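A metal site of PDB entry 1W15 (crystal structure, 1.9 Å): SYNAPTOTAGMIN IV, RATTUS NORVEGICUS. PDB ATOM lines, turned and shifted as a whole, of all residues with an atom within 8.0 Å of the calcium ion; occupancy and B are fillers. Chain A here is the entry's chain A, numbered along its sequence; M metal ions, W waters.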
ATOM      1  N   LEU A  50      19.250  16.604  14.336  1.00  0.00           N
ATOM      2  CA  LEU A  50      18.826  17.691  13.436  1.00  0.00           C
ATOM      3  C   LEU A  50      17.505  17.395  12.708  1.00  0.00           C
ATOM      4  O   LEU A  50      17.154  16.238  12.432  1.00  0.00           O
ATOM      5  CB  LEU A  50      19.940  18.057  12.444  1.00  0.00           C
ATOM      6  CG  LEU A  50      21.096  18.917  12.968  1.00  0.00           C
ATOM      7  CD1 LEU A  50      22.327  18.828  12.068  1.00  0.00           C
ATOM      8  CD2 LEU A  50      20.645  20.359  13.097  1.00  0.00           C
ATOM      9  N   SER A  51      16.772  18.446  12.433  1.00  0.00           N
ATOM     10  CA  SER A  51      15.460  18.280  11.848  1.00  0.00           C
ATOM     11  C   SER A  51      15.601  18.207  10.328  1.00  0.00           C
ATOM     12  O   SER A  51      16.686  18.499   9.779  1.00  0.00           O
ATOM     13  CB  SER A  51      14.539  19.395  12.320  1.00  0.00           C
ATOM     14  OG  SER A  51      14.886  20.649  11.707  1.00  0.00           O
ATOM     15  N   ASP A  52      14.524  17.786   9.672  1.00  0.00           N
ATOM     16  CA  ASP A  52      14.421  17.722   8.213  1.00  0.00           C
ATOM     17  C   ASP A  52      13.297  18.652   7.831  1.00  0.00           C
ATOM     18  O   ASP A  52      12.180  18.175   7.629  1.00  0.00           O
ATOM     19  CB  ASP A  52      14.063  16.294   7.799  1.00  0.00           C
ATOM     20  CG  ASP A  52      15.083  15.307   8.293  1.00  0.00           C
ATOM     21  OD1 ASP A  52      16.264  15.470   7.982  1.00  0.00           O
ATOM     22  OD2 ASP A  52      14.798  14.347   9.026  1.00  0.00           O
ATOM     23  N   PRO A  53      13.554  19.975   7.803  1.00  0.00           N
ATOM     24  CA  PRO A  53      12.468  20.950   7.665  1.00  0.00           C
ATOM     25  C   PRO A  53      11.810  21.076   6.290  1.00  0.00           C
ATOM     26  O   PRO A  53      12.475  20.953   5.282  1.00  0.00           O
ATOM     27  CB  PRO A  53      13.107  22.291   8.063  1.00  0.00           C
ATOM     28  CG  PRO A  53      14.622  22.080   7.789  1.00  0.00           C
ATOM     29  CD  PRO A  53      14.871  20.630   8.010  1.00  0.00           C
ATOM     30  N   VAL A  73      11.293  19.139   1.220  1.00  0.00           N
ATOM     31  CA  VAL A  73      11.972  19.101   2.510  1.00  0.00           C
ATOM     32  C   VAL A  73      13.486  19.142   2.338  1.00  0.00           C
ATOM     33  O   VAL A  73      14.056  18.516   1.448  1.00  0.00           O
ATOM     34  CB  VAL A  73      11.554  17.858   3.311  1.00  0.00           C
ATOM     35  CG1 VAL A  73      10.684  16.947   2.469  1.00  0.00           C
ATOM     36  CG2 VAL A  73      12.775  17.103   3.802  1.00  0.00           C
ATOM     37  N   LYS A  74      14.131  19.883   3.249  1.00  0.00           N
ATOM     38  CA  LYS A  74      15.589  19.894   3.334  1.00  0.00           C
ATOM     39  C   LYS A  74      16.022  18.935   4.464  1.00  0.00           C
ATOM     40  O   LYS A  74      15.450  18.965   5.549  1.00  0.00           O
ATOM     41  CB  LYS A  74      16.052  21.333   3.530  1.00  0.00           C
ATOM     42  CG  LYS A  74      15.628  22.224   2.346  1.00  0.00           C
ATOM     43  CD  LYS A  74      16.192  21.637   1.036  1.00  0.00           C
ATOM     44  CE  LYS A  74      16.027  22.525  -0.221  1.00  0.00           C
ATOM     45  NZ  LYS A  74      14.723  22.284  -0.918  1.00  0.00           N
ATOM     46  N   LYS A  75      16.969  18.041   4.199  1.00  0.00           N
ATOM     47  CA  LYS A  75      17.312  16.981   5.177  1.00  0.00           C
ATOM     48  C   LYS A  75      18.365  17.382   6.240  1.00  0.00           C
ATOM     49  O   LYS A  75      19.396  17.993   5.911  1.00  0.00           O
ATOM     50  CB  LYS A  75      17.778  15.701   4.456  1.00  0.00           C
ATOM     51  CG  LYS A  75      16.650  14.932   3.755  1.00  0.00           C
ATOM     52  CD  LYS A  75      17.254  13.806   2.877  1.00  0.00           C
ATOM     53  CE  LYS A  75      16.384  12.545   2.850  1.00  0.00           C
ATOM     54  NZ  LYS A  75      17.059  11.442   2.092  1.00  0.00           N
ATOM     55  N   CYS A  76      18.071  17.038   7.496  1.00  0.00           N
ATOM     56  CA  CYS A  76      19.027  17.094   8.628  1.00  0.00           C
ATOM     57  C   CYS A  76      19.856  18.391   8.740  1.00  0.00           C
ATOM     58  O   CYS A  76      21.103  18.374   8.532  1.00  0.00           O
ATOM     59  CB  CYS A  76      19.929  15.853   8.587  1.00  0.00           C
ATOM     60  SG  CYS A  76      20.977  15.635  10.053  1.00  0.00           S
ATOM     61  N   LEU A 105       7.906  22.509   9.734  1.00  0.00           N
ATOM     62  CA  LEU A 105       7.635  21.155  10.227  1.00  0.00           C
ATOM     63  C   LEU A 105       8.841  20.303   9.997  1.00  0.00           C
ATOM     64  O   LEU A 105       9.609  20.542   9.058  1.00  0.00           O
ATOM     65  CB  LEU A 105       6.452  20.551   9.447  1.00  0.00           C
ATOM     66  CG  LEU A 105       5.130  21.330   9.679  1.00  0.00           C
ATOM     67  CD1 LEU A 105       4.467  21.772   8.396  1.00  0.00           C
ATOM     68  CD2 LEU A 105       4.266  20.325  10.453  1.00  0.00           C
ATOM     69  N   ASP A 106       8.984  19.270  10.828  1.00  0.00           N
ATOM     70  CA  ASP A 106      10.087  18.349  10.688  1.00  0.00           C
ATOM     71  C   ASP A 106       9.502  17.091  10.039  1.00  0.00           C
ATOM     72  O   ASP A 106       8.576  16.475  10.590  1.00  0.00           O
ATOM     73  CB  ASP A 106      10.644  18.046  12.070  1.00  0.00           C
ATOM     74  CG  ASP A 106      11.693  16.985  12.067  1.00  0.00           C
ATOM     75  OD1 ASP A 106      12.473  16.852  11.103  1.00  0.00           O
ATOM     76  OD2 ASP A 106      11.790  16.196  13.005  1.00  0.00           O
ATOM     77  N   SER A 107      10.009  16.747   8.855  1.00  0.00           N
ATOM     78  CA  SER A 107       9.559  15.547   8.187  1.00  0.00           C
ATOM     79  C   SER A 107      10.130  14.314   8.868  1.00  0.00           C
ATOM     80  O   SER A 107      11.343  14.180   9.024  1.00  0.00           O
ATOM     81  CB  SER A 107       9.952  15.614   6.705  1.00  0.00           C
ATOM     82  OG  SER A 107       9.728  14.379   6.096  1.00  0.00           O
ATOM     83  N   GLU A 108       9.250  13.420   9.312  1.00  0.00           N
ATOM     84  CA  GLU A 108       9.713  12.244  10.050  1.00  0.00           C
ATOM     85  C   GLU A 108       8.866  11.067   9.593  1.00  0.00           C
ATOM     86  O   GLU A 108       7.645  11.092   9.770  1.00  0.00           O
ATOM     87  CB  GLU A 108       9.545  12.447  11.561  1.00  0.00           C
ATOM     88  CG  GLU A 108      10.108  11.281  12.382  1.00  0.00           C
ATOM     89  CD  GLU A 108      11.618  11.360  12.568  1.00  0.00           C
ATOM     90  OE1 GLU A 108      12.170  12.462  12.445  1.00  0.00           O
ATOM     91  OE2 GLU A 108      12.262  10.334  12.840  1.00  0.00           O
ATOM     92  N   ARG A 109       9.470  10.033   9.051  1.00  0.00           N
ATOM     93  CA  ARG A 109       8.708   8.864   8.625  1.00  0.00           C
ATOM     94  C   ARG A 109       8.177   8.112   9.838  1.00  0.00           C
ATOM     95  O   ARG A 109       8.921   7.845  10.794  1.00  0.00           O
ATOM     96  CB  ARG A 109       9.585   7.906   7.772  1.00  0.00           C
ATOM     97  CG  ARG A 109      10.085   8.533   6.441  1.00  0.00           C
ATOM     98  CD  ARG A 109      11.032   7.578   5.631  1.00  0.00           C
ATOM     99  NE  ARG A 109      12.026   8.231   4.739  1.00  0.00           N
ATOM    100  CZ  ARG A 109      12.147   9.550   4.426  1.00  0.00           C
ATOM    101  NH1 ARG A 109      11.327  10.472   4.923  1.00  0.00           N
ATOM    102  NH2 ARG A 109      13.126   9.939   3.596  1.00  0.00           N
ATOM    103  N   SER A 111       5.622   8.736  11.969  1.00  0.00           N
ATOM    104  CA  SER A 111       4.964   9.571  13.018  1.00  0.00           C
ATOM    105  C   SER A 111       4.436  10.869  12.459  1.00  0.00           C
ATOM    106  O   SER A 111       4.845  11.286  11.389  1.00  0.00           O
ATOM    107  CB  SER A 111       5.910   9.933  14.162  1.00  0.00           C
ATOM    108  OG  SER A 111       7.071  10.568  13.619  1.00  0.00           O
ATOM    109  N   ASN A 113       4.374  14.616  11.655  1.00  0.00           N
ATOM    110  CA  ASN A 113       5.466  15.588  11.544  1.00  0.00           C
ATOM    111  C   ASN A 113       5.234  16.709  12.566  1.00  0.00           C
ATOM    112  O   ASN A 113       4.144  17.245  12.661  1.00  0.00           O
ATOM    113  CB  ASN A 113       5.499  16.195  10.138  1.00  0.00           C
ATOM    114  CG  ASN A 113       5.915  15.164   9.091  1.00  0.00           C
ATOM    115  OD1 ASN A 113       6.415  14.103   9.415  1.00  0.00           O
ATOM    116  ND2 ASN A 113       5.691  15.486   7.830  1.00  0.00           N
ATOM    117  N   GLU A 114       6.252  17.040  13.343  1.00  0.00           N
ATOM    118  CA  GLU A 114       6.093  18.014  14.426  1.00  0.00           C
ATOM    119  C   GLU A 114       6.238  19.417  13.893  1.00  0.00           C
ATOM    120  O   GLU A 114       7.001  19.654  12.945  1.00  0.00           O
ATOM    121  CB  GLU A 114       7.171  17.741  15.474  1.00  0.00           C
ATOM    122  CG  GLU A 114       7.298  18.840  16.530  1.00  0.00           C
ATOM    123  CD  GLU A 114       7.875  18.273  17.828  1.00  0.00           C
ATOM    124  OE1 GLU A 114       8.461  17.183  17.752  1.00  0.00           O
ATOM    125  OE2 GLU A 114       7.702  18.887  18.910  1.00  0.00           O
ATOM    126  N   ILE A 116       7.765  22.808  14.099  1.00  0.00           N
ATOM    127  CA  ILE A 116       8.971  23.360  14.712  1.00  0.00           C
ATOM    128  C   ILE A 116       8.700  24.823  15.106  1.00  0.00           C
ATOM    129  O   ILE A 116       9.154  25.308  16.160  1.00  0.00           O
ATOM    130  CB  ILE A 116      10.128  23.344  13.681  1.00  0.00           C
ATOM    131  CG1 ILE A 116      10.599  21.921  13.346  1.00  0.00           C
ATOM    132  CG2 ILE A 116      11.327  24.206  14.141  1.00  0.00           C
ATOM    133  CD1 ILE A 116      11.602  21.916  12.134  1.00  0.00           C
HETATM  134 CA    CA M   1      13.197  14.283  10.932  1.00  0.00          CA
HETATM  135  O   HOH W   1      14.640  12.356  12.258  1.00  0.00           O
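The side-chain carboxylate (OD1) of Asp 52 sits at hydrogen-bond distance from the backbone NH (N) of Cys 76 (2.4 Å).
The side-chain amide oxygen of Asn 113 sits at hydrogen-bond distance from the backbone NH of Glu 108, at 2.9 Å.
The backbone carbonyl oxygen of Asp 106 lies close to the side-chain amide oxygen of Asn 113 (3.4 Å).
O of Glu 114 sits at hydrogen-bond distance from N of Asp 106 (2.9 Å).
The calcium ion is bound by the side-chain carboxylate of Asp 52, the side-chain carboxylate of Glu 108, the backbone carbonyl oxygen of Ser 107, the side-chain carboxylate of Asp 106 and water W1.
Four residues have an atom within 4 Å of the calcium ion: Asp 52, Asp 106, Ser 107 and Glu 108.
The nearest printed residue that does not touch the calcium ion is Ser 51 (4.6 Å).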
